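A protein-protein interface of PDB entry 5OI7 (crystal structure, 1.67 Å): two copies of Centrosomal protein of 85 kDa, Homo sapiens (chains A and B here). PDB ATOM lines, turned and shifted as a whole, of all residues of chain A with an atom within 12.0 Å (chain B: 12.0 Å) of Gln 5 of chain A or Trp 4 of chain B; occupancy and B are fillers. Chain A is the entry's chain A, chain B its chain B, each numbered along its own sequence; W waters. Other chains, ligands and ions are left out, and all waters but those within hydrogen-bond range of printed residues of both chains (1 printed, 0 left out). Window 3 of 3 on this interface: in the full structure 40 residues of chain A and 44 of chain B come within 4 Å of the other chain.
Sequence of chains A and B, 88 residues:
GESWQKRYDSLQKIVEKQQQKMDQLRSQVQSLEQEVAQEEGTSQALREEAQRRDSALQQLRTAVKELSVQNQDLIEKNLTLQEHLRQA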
ATOM      1  N   GLY A   1       5.611 -26.702 -33.752  1.00  0.00           N
ATOM      2  CA  GLY A   1       6.118 -25.740 -32.790  1.00  0.00           C
ATOM      3  C   GLY A   1       7.456 -25.160 -33.201  1.00  0.00           C
ATOM      4  O   GLY A   1       7.645 -24.767 -34.350  1.00  0.00           O
ATOM      5  N   GLU A   2       8.393 -25.107 -32.260  1.00  0.00           N
ATOM      6  CA  GLU A   2       9.728 -24.616 -32.561  1.00  0.00           C
ATOM      7  C   GLU A   2      10.516 -25.668 -33.332  1.00  0.00           C
ATOM      8  O   GLU A   2      10.421 -26.866 -33.053  1.00  0.00           O
ATOM      9  CB  GLU A   2      10.460 -24.249 -31.272  1.00  0.00           C
ATOM     10  CG  GLU A   2       9.651 -23.351 -30.355  1.00  0.00           C
ATOM     11  CD  GLU A   2       9.793 -23.735 -28.896  1.00  0.00           C
ATOM     12  OE1 GLU A   2      10.884 -23.521 -28.329  1.00  0.00           O
ATOM     13  OE2 GLU A   2       8.816 -24.268 -28.323  1.00  0.00           O
ATOM     14  N   SER A   3      11.292 -25.211 -34.310  1.00  0.00           N
ATOM     15  CA  SER A   3      12.154 -26.118 -35.048  1.00  0.00           C
ATOM     16  C   SER A   3      13.201 -26.712 -34.113  1.00  0.00           C
ATOM     17  O   SER A   3      13.441 -26.216 -33.009  1.00  0.00           O
ATOM     18  CB  SER A   3      12.843 -25.392 -36.204  1.00  0.00           C
ATOM     19  OG  SER A   3      13.753 -24.419 -35.717  1.00  0.00           O
ATOM     20  N   TRP A   4      13.833 -27.792 -34.573  1.00  0.00           N
ATOM     21  CA  TRP A   4      14.906 -28.380 -33.779  1.00  0.00           C
ATOM     22  C   TRP A   4      16.107 -27.453 -33.693  1.00  0.00           C
ATOM     23  O   TRP A   4      16.781 -27.412 -32.656  1.00  0.00           O
ATOM     24  CB  TRP A   4      15.298 -29.744 -34.349  1.00  0.00           C
ATOM     25  CG  TRP A   4      14.337 -30.811 -33.940  1.00  0.00           C
ATOM     26  CD1 TRP A   4      13.425 -31.448 -34.732  1.00  0.00           C
ATOM     27  CD2 TRP A   4      14.165 -31.344 -32.621  1.00  0.00           C
ATOM     28  NE1 TRP A   4      12.708 -32.358 -33.991  1.00  0.00           N
ATOM     29  CE2 TRP A   4      13.141 -32.311 -32.691  1.00  0.00           C
ATOM     30  CE3 TRP A   4      14.782 -31.098 -31.387  1.00  0.00           C
ATOM     31  CZ2 TRP A   4      12.721 -33.035 -31.575  1.00  0.00           C
ATOM     32  CZ3 TRP A   4      14.363 -31.819 -30.280  1.00  0.00           C
ATOM     33  CH2 TRP A   4      13.344 -32.774 -30.382  1.00  0.00           C
ATOM     34  N   GLN A   5      16.387 -26.695 -34.756  1.00  0.00           N
ATOM     35  CA  GLN A   5      17.422 -25.669 -34.674  1.00  0.00           C
ATOM     36  C   GLN A   5      17.123 -24.674 -33.559  1.00  0.00           C
ATOM     37  O   GLN A   5      18.015 -24.311 -32.784  1.00  0.00           O
ATOM     38  CB  GLN A   5      17.553 -24.943 -36.014  1.00  0.00           C
ATOM     39  CG  GLN A   5      18.545 -23.792 -35.992  1.00  0.00           C
ATOM     40  CD  GLN A   5      18.516 -22.969 -37.267  1.00  0.00           C
ATOM     41  OE1 GLN A   5      19.155 -23.315 -38.259  1.00  0.00           O
ATOM     42  NE2 GLN A   5      17.766 -21.872 -37.245  1.00  0.00           N
ATOM     43  N   LYS A   6      15.870 -24.219 -33.461  1.00  0.00           N
ATOM     44  CA  LYS A   6      15.520 -23.257 -32.418  1.00  0.00           C
ATOM     45  C   LYS A   6      15.598 -23.889 -31.036  1.00  0.00           C
ATOM     46  O   LYS A   6      16.010 -23.234 -30.072  1.00  0.00           O
ATOM     47  CB  LYS A   6      14.121 -22.696 -32.654  1.00  0.00           C
ATOM     48  CG  LYS A   6      13.652 -21.778 -31.532  1.00  0.00           C
ATOM     49  CD  LYS A   6      14.374 -20.440 -31.583  1.00  0.00           C
ATOM     50  CE  LYS A   6      14.536 -19.825 -30.196  1.00  0.00           C
ATOM     51  NZ  LYS A   6      15.499 -20.591 -29.349  1.00  0.00           N
ATOM     52  N   ARG A   7      15.180 -25.148 -30.911  1.00  0.00           N
ATOM     53  CA  ARG A   7      15.298 -25.829 -29.626  1.00  0.00           C
ATOM     54  C   ARG A   7      16.761 -26.034 -29.257  1.00  0.00           C
ATOM     55  O   ARG A   7      17.140 -25.916 -28.086  1.00  0.00           O
ATOM     56  CB  ARG A   7      14.550 -27.160 -29.672  1.00  0.00           C
ATOM     57  CG  ARG A   7      13.060 -27.007 -29.942  1.00  0.00           C
ATOM     58  CD  ARG A   7      12.389 -28.360 -30.056  1.00  0.00           C
ATOM     59  NE  ARG A   7      10.995 -28.246 -30.469  1.00  0.00           N
ATOM     60  CZ  ARG A   7       9.957 -28.295 -29.641  1.00  0.00           C
ATOM     61  NH1 ARG A   7      10.149 -28.452 -28.340  1.00  0.00           N
ATOM     62  NH2 ARG A   7       8.721 -28.192 -30.123  1.00  0.00           N
ATOM     63  N   TYR A   8      17.601 -26.329 -30.251  1.00  0.00           N
ATOM     64  CA  TYR A   8      19.040 -26.392 -30.015  1.00  0.00           C
ATOM     65  C   TYR A   8      19.560 -25.066 -29.472  1.00  0.00           C
ATOM     66  O   TYR A   8      20.313 -25.035 -28.492  1.00  0.00           O
ATOM     67  CB  TYR A   8      19.763 -26.759 -31.313  1.00  0.00           C
ATOM     68  CG  TYR A   8      21.273 -26.765 -31.204  1.00  0.00           C
ATOM     69  CD1 TYR A   8      22.011 -25.608 -31.417  1.00  0.00           C
ATOM     70  CD2 TYR A   8      21.959 -27.932 -30.898  1.00  0.00           C
ATOM     71  CE1 TYR A   8      23.395 -25.616 -31.323  1.00  0.00           C
ATOM     72  CE2 TYR A   8      23.334 -27.950 -30.806  1.00  0.00           C
ATOM     73  CZ  TYR A   8      24.047 -26.793 -31.018  1.00  0.00           C
ATOM     74  OH  TYR A   8      25.419 -26.819 -30.920  1.00  0.00           O
ATOM     75  N   ASP A   9      19.176 -23.956 -30.112  1.00  0.00           N
ATOM     76  CA  ASP A   9      19.628 -22.643 -29.658  1.00  0.00           C
ATOM     77  C   ASP A   9      19.211 -22.377 -28.217  1.00  0.00           C
ATOM     78  O   ASP A   9      19.977 -21.797 -27.439  1.00  0.00           O
ATOM     79  CB  ASP A   9      19.083 -21.542 -30.568  1.00  0.00           C
ATOM     80  CG  ASP A   9      19.781 -21.490 -31.914  1.00  0.00           C
ATOM     81  OD1 ASP A   9      20.919 -21.994 -32.026  1.00  0.00           O
ATOM     82  OD2 ASP A   9      19.181 -20.934 -32.859  1.00  0.00           O
ATOM     83  N   SER A  10      17.987 -22.767 -27.852  1.00  0.00           N
ATOM     84  CA  SER A  10      17.534 -22.583 -26.474  1.00  0.00           C
ATOM     85  C   SER A  10      18.356 -23.431 -25.515  1.00  0.00           C
ATOM     86  O   SER A  10      18.714 -22.977 -24.421  1.00  0.00           O
ATOM     87  CB  SER A  10      16.049 -22.931 -26.354  1.00  0.00           C
ATOM     88  OG  SER A  10      15.232 -21.941 -26.954  1.00  0.00           O
ATOM     89  N   LEU A  11      18.657 -24.670 -25.907  1.00  0.00           N
ATOM     90  CA  LEU A  11      19.481 -25.530 -25.066  1.00  0.00           C
ATOM     91  C   LEU A  11      20.894 -24.975 -24.938  1.00  0.00           C
ATOM     92  O   LEU A  11      21.509 -25.069 -23.870  1.00  0.00           O
ATOM     93  CB  LEU A  11      19.498 -26.952 -25.630  1.00  0.00           C
ATOM     94  CG  LEU A  11      19.961 -28.061 -24.679  1.00  0.00           C
ATOM     95  CD1 LEU A  11      19.120 -28.050 -23.410  1.00  0.00           C
ATOM     96  CD2 LEU A  11      19.907 -29.429 -25.349  1.00  0.00           C
ATOM     97  N   GLN A  12      21.421 -24.371 -26.010  1.00  0.00           N
ATOM     98  CA  GLN A  12      22.773 -23.823 -25.947  1.00  0.00           C
ATOM     99  C   GLN A  12      22.855 -22.641 -24.992  1.00  0.00           C
ATOM    100  O   GLN A  12      23.901 -22.415 -24.374  1.00  0.00           O
ATOM    101  CB  GLN A  12      23.250 -23.412 -27.342  1.00  0.00           C
ATOM    102  CG  GLN A  12      24.556 -22.623 -27.356  1.00  0.00           C
ATOM    103  CD  GLN A  12      25.751 -23.434 -26.877  1.00  0.00           C
ATOM    104  OE1 GLN A  12      25.742 -24.661 -26.927  1.00  0.00           O
ATOM    105  NE2 GLN A  12      26.788 -22.742 -26.408  1.00  0.00           N
ATOM    106  N   LYS A  13      21.773 -21.869 -24.861  1.00  0.00           N
ATOM    107  CA  LYS A  13      21.759 -20.811 -23.854  1.00  0.00           C
ATOM    108  C   LYS A  13      21.889 -21.397 -22.455  1.00  0.00           C
ATOM    109  O   LYS A  13      22.536 -20.808 -21.580  1.00  0.00           O
ATOM    110  CB  LYS A  13      20.481 -19.980 -23.972  1.00  0.00           C
ATOM    111  CG  LYS A  13      20.347 -19.237 -25.294  1.00  0.00           C
ATOM    112  CD  LYS A  13      18.947 -18.675 -25.473  1.00  0.00           C
ATOM    113  CE  LYS A  13      18.644 -17.638 -24.420  1.00  0.00           C
ATOM    114  NZ  LYS A  13      17.212 -17.233 -24.393  1.00  0.00           N
ATOM    115  N   ILE A  14      21.286 -22.566 -22.229  1.00  0.00           N
ATOM    116  CA  ILE A  14      21.414 -23.231 -20.936  1.00  0.00           C
ATOM    117  C   ILE A  14      22.847 -23.701 -20.716  1.00  0.00           C
ATOM    118  O   ILE A  14      23.406 -23.550 -19.623  1.00  0.00           O
ATOM    119  CB  ILE A  14      20.407 -24.392 -20.842  1.00  0.00           C
ATOM    120  CG1 ILE A  14      18.988 -23.847 -20.672  1.00  0.00           C
ATOM    121  CG2 ILE A  14      20.762 -25.330 -19.696  1.00  0.00           C
ATOM    122  CD1 ILE A  14      17.908 -24.898 -20.807  1.00  0.00           C
ATOM    123  N   VAL A  15      23.468 -24.275 -21.750  1.00  0.00           N
ATOM    124  CA  VAL A  15      24.870 -24.675 -21.648  1.00  0.00           C
ATOM    125  C   VAL A  15      25.740 -23.488 -21.248  1.00  0.00           C
ATOM    126  O   VAL A  15      26.629 -23.607 -20.393  1.00  0.00           O
ATOM    127  CB  VAL A  15      25.340 -25.299 -22.977  1.00  0.00           C
ATOM    128  CG1 VAL A  15      26.853 -25.416 -23.012  1.00  0.00           C
ATOM    129  CG2 VAL A  15      24.685 -26.656 -23.187  1.00  0.00           C
ATOM    130  N   GLU A  16      25.505 -22.326 -21.862  1.00  0.00           N
ATOM    131  CA  GLU A  16      26.320 -21.152 -21.563  1.00  0.00           C
ATOM    132  C   GLU A  16      26.063 -20.637 -20.152  1.00  0.00           C
ATOM    133  O   GLU A  16      27.004 -20.274 -19.436  1.00  0.00           O
ATOM    134  CB  GLU A  16      26.053 -20.060 -22.602  1.00  0.00           C
ATOM    135  CG  GLU A  16      26.539 -20.445 -23.994  1.00  0.00           C
ATOM    136  CD  GLU A  16      26.117 -19.463 -25.072  1.00  0.00           C
ATOM    137  OE1 GLU A  16      25.453 -18.454 -24.752  1.00  0.00           O
ATOM    138  OE2 GLU A  16      26.454 -19.708 -26.247  1.00  0.00           O
ATOM    139  N   GLY B   1      25.222 -34.273 -43.006  1.00  0.00           N
ATOM    140  CA  GLY B   1      25.552 -33.802 -41.675  1.00  0.00           C
ATOM    141  C   GLY B   1      24.532 -34.263 -40.655  1.00  0.00           C
ATOM    142  O   GLY B   1      23.558 -34.932 -40.999  1.00  0.00           O
ATOM    143  N   GLU B   2      24.754 -33.912 -39.392  1.00  0.00           N
ATOM    144  CA  GLU B   2      23.814 -34.277 -38.344  1.00  0.00           C
ATOM    145  C   GLU B   2      22.605 -33.353 -38.364  1.00  0.00           C
ATOM    146  O   GLU B   2      22.728 -32.149 -38.604  1.00  0.00           O
ATOM    147  CB  GLU B   2      24.489 -34.217 -36.977  1.00  0.00           C
ATOM    148  CG  GLU B   2      25.487 -35.329 -36.739  1.00  0.00           C
ATOM    149  CD  GLU B   2      26.191 -35.189 -35.409  1.00  0.00           C
ATOM    150  OE1 GLU B   2      26.169 -34.075 -34.846  1.00  0.00           O
ATOM    151  OE2 GLU B   2      26.760 -36.190 -34.925  1.00  0.00           O
ATOM    152  N   SER B   3      21.433 -33.927 -38.114  1.00  0.00           N
ATOM    153  CA  SER B   3      20.231 -33.123 -37.981  1.00  0.00           C
ATOM    154  C   SER B   3      20.319 -32.261 -36.726  1.00  0.00           C
ATOM    155  O   SER B   3      21.088 -32.539 -35.802  1.00  0.00           O
ATOM    156  CB  SER B   3      18.991 -34.010 -37.913  1.00  0.00           C
ATOM    157  OG  SER B   3      18.952 -34.736 -36.695  1.00  0.00           O
ATOM    158  N   TRP B   4      19.519 -31.195 -36.700  1.00  0.00           N
ATOM    159  CA  TRP B   4      19.461 -30.382 -35.492  1.00  0.00           C
ATOM    160  C   TRP B   4      18.906 -31.176 -34.320  1.00  0.00           C
ATOM    161  O   TRP B   4      19.303 -30.943 -33.173  1.00  0.00           O
ATOM    162  CB  TRP B   4      18.635 -29.121 -35.734  1.00  0.00           C
ATOM    163  CG  TRP B   4      19.337 -28.140 -36.601  1.00  0.00           C
ATOM    164  CD1 TRP B   4      19.113 -27.910 -37.928  1.00  0.00           C
ATOM    165  CD2 TRP B   4      20.405 -27.266 -36.217  1.00  0.00           C
ATOM    166  NE1 TRP B   4      19.968 -26.940 -38.390  1.00  0.00           N
ATOM    167  CE2 TRP B   4      20.771 -26.527 -37.359  1.00  0.00           C
ATOM    168  CE3 TRP B   4      21.082 -27.033 -35.015  1.00  0.00           C
ATOM    169  CZ2 TRP B   4      21.785 -25.571 -37.336  1.00  0.00           C
ATOM    170  CZ3 TRP B   4      22.088 -26.082 -34.995  1.00  0.00           C
ATOM    171  CH2 TRP B   4      22.429 -25.363 -36.147  1.00  0.00           C
ATOM    172  N   GLN B   5      17.995 -32.116 -34.581  1.00  0.00           N
ATOM    173  CA  GLN B   5      17.490 -32.951 -33.499  1.00  0.00           C
ATOM    174  C   GLN B   5      18.600 -33.809 -32.905  1.00  0.00           C
ATOM    175  O   GLN B   5      18.687 -33.957 -31.681  1.00  0.00           O
ATOM    176  CB  GLN B   5      16.343 -33.831 -33.988  1.00  0.00           C
ATOM    177  CG  GLN B   5      15.804 -34.750 -32.902  1.00  0.00           C
ATOM    178  CD  GLN B   5      14.648 -35.609 -33.365  1.00  0.00           C
ATOM    179  OE1 GLN B   5      14.261 -35.589 -34.539  1.00  0.00           O
ATOM    180  NE2 GLN B   5      14.082 -36.372 -32.440  1.00  0.00           N
ATOM    181  N   LYS B   6      19.460 -34.376 -33.754  1.00  0.00           N
ATOM    182  CA  LYS B   6      20.584 -35.160 -33.254  1.00  0.00           C
ATOM    183  C   LYS B   6      21.555 -34.281 -32.475  1.00  0.00           C
ATOM    184  O   LYS B   6      22.054 -34.681 -31.414  1.00  0.00           O
ATOM    185  CB  LYS B   6      21.292 -35.861 -34.416  1.00  0.00           C
ATOM    186  CG  LYS B   6      22.698 -36.362 -34.092  1.00  0.00           C
ATOM    187  CD  LYS B   6      22.688 -37.520 -33.101  1.00  0.00           C
ATOM    188  CE  LYS B   6      24.108 -37.969 -32.783  1.00  0.00           C
ATOM    189  NZ  LYS B   6      24.145 -39.178 -31.917  1.00  0.00           N
ATOM    190  N   ARG B   7      21.822 -33.071 -32.976  1.00  0.00           N
ATOM    191  CA  ARG B   7      22.688 -32.146 -32.250  1.00  0.00           C
ATOM    192  C   ARG B   7      22.064 -31.739 -30.922  1.00  0.00           C
ATOM    193  O   ARG B   7      22.772 -31.546 -29.925  1.00  0.00           O
ATOM    194  CB  ARG B   7      22.970 -30.906 -33.094  1.00  0.00           C
ATOM    195  CG  ARG B   7      23.717 -31.167 -34.389  1.00  0.00           C
ATOM    196  CD  ARG B   7      23.773 -29.896 -35.214  1.00  0.00           C
ATOM    197  NE  ARG B   7      24.507 -30.076 -36.462  1.00  0.00           N
ATOM    198  CZ  ARG B   7      24.393 -29.271 -37.513  1.00  0.00           C
ATOM    199  NH1 ARG B   7      23.565 -28.236 -37.470  1.00  0.00           N
ATOM    200  NH2 ARG B   7      25.097 -29.507 -38.610  1.00  0.00           N
ATOM    201  N   TYR B   8      20.741 -31.571 -30.898  1.00  0.00           N
ATOM    202  CA  TYR B   8      20.052 -31.307 -29.640  1.00  0.00           C
ATOM    203  C   TYR B   8      20.281 -32.446 -28.655  1.00  0.00           C
ATOM    204  O   TYR B   8      20.597 -32.219 -27.481  1.00  0.00           O
ATOM    205  CB  TYR B   8      18.557 -31.102 -29.904  1.00  0.00           C
ATOM    206  CG  TYR B   8      17.734 -30.835 -28.666  1.00  0.00           C
ATOM    207  CD1 TYR B   8      17.316 -31.877 -27.842  1.00  0.00           C
ATOM    208  CD2 TYR B   8      17.360 -29.542 -28.328  1.00  0.00           C
ATOM    209  CE1 TYR B   8      16.563 -31.634 -26.707  1.00  0.00           C
ATOM    210  CE2 TYR B   8      16.604 -29.289 -27.191  1.00  0.00           C
ATOM    211  CZ  TYR B   8      16.210 -30.339 -26.388  1.00  0.00           C
ATOM    212  OH  TYR B   8      15.462 -30.095 -25.258  1.00  0.00           O
ATOM    213  N   ASP B   9      20.141 -33.687 -29.126  1.00  0.00           N
ATOM    214  CA  ASP B   9      20.324 -34.833 -28.243  1.00  0.00           C
ATOM    215  C   ASP B   9      21.744 -34.880 -27.685  1.00  0.00           C
ATOM    216  O   ASP B   9      21.945 -35.217 -26.511  1.00  0.00           O
ATOM    217  CB  ASP B   9      19.987 -36.123 -28.990  1.00  0.00           C
ATOM    218  CG  ASP B   9      20.061 -37.347 -28.101  1.00  0.00           C
ATOM    219  OD1 ASP B   9      19.196 -37.490 -27.214  1.00  0.00           O
ATOM    220  OD2 ASP B   9      20.982 -38.167 -28.291  1.00  0.00           O
ATOM    221  N   SER B  10      22.742 -34.548 -28.507  1.00  0.00           N
ATOM    222  CA  SER B  10      24.119 -34.530 -28.017  1.00  0.00           C
ATOM    223  C   SER B  10      24.347 -33.368 -27.059  1.00  0.00           C
ATOM    224  O   SER B  10      25.120 -33.489 -26.101  1.00  0.00           O
ATOM    225  CB  SER B  10      25.101 -34.450 -29.186  1.00  0.00           C
ATOM    226  OG  SER B  10      24.981 -35.579 -30.032  1.00  0.00           O
ATOM    227  N   LEU B  11      23.691 -32.232 -27.303  1.00  0.00           N
ATOM    228  CA  LEU B  11      23.871 -31.084 -26.423  1.00  0.00           C
ATOM    229  C   LEU B  11      23.234 -31.320 -25.060  1.00  0.00           C
ATOM    230  O   LEU B  11      23.745 -30.830 -24.046  1.00  0.00           O
ATOM    231  CB  LEU B  11      23.293 -29.829 -27.075  1.00  0.00           C
ATOM    232  CG  LEU B  11      23.754 -28.493 -26.492  1.00  0.00           C
ATOM    233  CD1 LEU B  11      25.267 -28.372 -26.573  1.00  0.00           C
ATOM    234  CD2 LEU B  11      23.082 -27.334 -27.211  1.00  0.00           C
ATOM    235  N   GLN B  12      22.123 -32.062 -25.017  1.00  0.00           N
ATOM    236  CA  GLN B  12      21.503 -32.385 -23.737  1.00  0.00           C
ATOM    237  C   GLN B  12      22.435 -33.223 -22.871  1.00  0.00           C
ATOM    238  O   GLN B  12      22.454 -33.077 -21.644  1.00  0.00           O
ATOM    239  CB  GLN B  12      20.173 -33.108 -23.964  1.00  0.00           C
ATOM    240  CG  GLN B  12      19.506 -33.612 -22.687  1.00  0.00           C
ATOM    241  CD  GLN B  12      19.081 -32.490 -21.758  1.00  0.00           C
ATOM    242  OE1 GLN B  12      18.756 -31.389 -22.202  1.00  0.00           O
ATOM    243  NE2 GLN B  12      19.083 -32.766 -20.458  1.00  0.00           N
ATOM    244  N   LYS B  13      23.221 -34.109 -23.490  1.00  0.00           N
ATOM    245  CA  LYS B  13      24.216 -34.858 -22.726  1.00  0.00           C
ATOM    246  C   LYS B  13      25.221 -33.920 -22.074  1.00  0.00           C
ATOM    247  O   LYS B  13      25.638 -34.137 -20.929  1.00  0.00           O
ATOM    248  CB  LYS B  13      24.929 -35.863 -23.629  1.00  0.00           C
ATOM    249  CG  LYS B  13      24.020 -36.942 -24.192  1.00  0.00           C
ATOM    250  CD  LYS B  13      24.740 -37.755 -25.251  1.00  0.00           C
ATOM    251  CE  LYS B  13      23.809 -38.762 -25.900  1.00  0.00           C
ATOM    252  NZ  LYS B  13      24.454 -39.425 -27.065  1.00  0.00           N
ATOM    253  N   ILE B  14      25.622 -32.867 -22.788  1.00  0.00           N
ATOM    254  CA  ILE B  14      26.517 -31.874 -22.204  1.00  0.00           C
ATOM    255  C   ILE B  14      25.838 -31.172 -21.037  1.00  0.00           C
ATOM    256  O   ILE B  14      26.451 -30.949 -19.985  1.00  0.00           O
ATOM    257  CB  ILE B  14      26.980 -30.873 -23.280  1.00  0.00           C
ATOM    258  CG1 ILE B  14      27.863 -31.577 -24.310  1.00  0.00           C
ATOM    259  CG2 ILE B  14      27.714 -29.695 -22.642  1.00  0.00           C
ATOM    260  CD1 ILE B  14      28.247 -30.703 -25.485  1.00  0.00           C
HETATM  261  O   HOH W   1      20.364 -24.914 -40.466  1.00  0.00           O
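Water W1 lies within hydrogen-bond range of NE1 of Trp 4 of chain B (2.9 Å) and OE1 of Gln 5 of chain A (3.0 Å).
Of the 14 printed residues of chain B, 6 touch a printed residue of chain A.
Printed residues of chain B that touch a printed residue of chain A: Trp 4, Gln 5, Arg 7, Tyr 8, Leu 11 and Gln 12.
Hydrophobic or aromatic side chains of chain B within 4 Å of the printed part of chain A: Trp 4, Tyr 8 and Leu 11.
Along chain B the printed residues that touch a printed residue of chain A span positions 4 to 12.
Of the 16 printed residues of chain A, 7 touch a printed residue of chain B.
Along chain A the printed residues that touch a printed residue of chain B span positions 4 to 15.
Among the printed residues, 14 pairs touch across the chains.
NE of Arg 7 of chain B is in hydrogen-bond range of O of Glu 2 of chain B, 3.5 Å away.
NE2 of Gln 12 of chain A lies within hydrogen-bond range of OE2 of Glu 16 of chain A (3.1 Å).
O of Glu 2 of chain A is in hydrogen-bond range of NE of Arg 7 of chain A (3.0 Å).
Trp 4 of chain A touches Gln 5 of chain B, and with the chains exchanged Gln 5 of chain A touches Trp 4 of chain B.
Arg 7 of chain A touches Tyr 8 of chain B, and with the chains exchanged Tyr 8 of chain A touches Arg 7 of chain B.
Tyr 8 of chain A touches its own counterpart, Tyr 8 of chain B.
Leu 11 of chain B touches its own counterpart, Leu 11 of chain A.
Of the 14 pairs that touch across the chains among the printed residues, 13 have their exchanged pair printed and touching as well.
C of Trp 4 of chain A touches CB of Trp 4 of chain B (3.7 Å).
Trp 4 of chain A touches Gln 5 of chain B (CD2 to CB, 3.6 Å).
Gln 5 of chain A touches Trp 4 of chain B (N to CB, 3.4 Å).
O of Arg 7 of chain A touches CE2 of Tyr 8 of chain B (3.5 Å).
CD1 of Tyr 8 of chain A touches CZ3 of Trp 4 of chain B (3.6 Å).
CE2 of Tyr 8 of chain A touches O of Arg 7 of chain B, at 3.7 Å.
N of Tyr 8 of chain A touches CD2 of Tyr 8 of chain B, at 3.8 Å.
CD2 of Leu 11 of chain B touches CE2 of Tyr 8 of chain A, 3.7 Å away.
CB of Leu 11 of chain B touches CD2 of Leu 11 of chain A, at 3.8 Å.
Gln 12 of chain B touches Leu 11 of chain A (N to CD2, 3.5 Å).
Of chain A, only Trp 4 (3.7 Å), Gln 5 (3.4 Å) and Tyr 8 (3.6 Å) come within 4 Å of Trp 4 of chain B.
No residue of chain B comes within 4 Å of Ser 3 of chain A.
Trp 4 of chain A touches just these residues of chain B: Trp 4, Gln 5 and Tyr 8.
No residue of chain B comes within 4 Å of Lys 6 of chain A.
Tyr 8 of chain A touches four residues of chain B.
No residue of chain B comes within 4 Å of Asp 9 of chain A.
Gln 5 of chain B touches one residue of chain A.
Of chain A, only Tyr 8 comes within 4 Å of Arg 7 of chain B.
Printed residues of chain A within 4 Å of Gln 12 of chain B: Leu 11 (3.5 Å).
Of the printed residues of chain B, Gln 12 of chain A touches Leu 11 (3.6 Å).
Of the printed residues of chain A, Tyr 8 of chain B touches Trp 4, Arg 7, Tyr 8 and Leu 11.
Glu 2 of chain B touches none of the printed residues of chain A.
Gly 1 of chain A touches none of the printed residues of chain B.
The nearest printed residue of chain B that does not touch Gln 12 of chain A is Ile 14 of chain B (6.7 Å).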
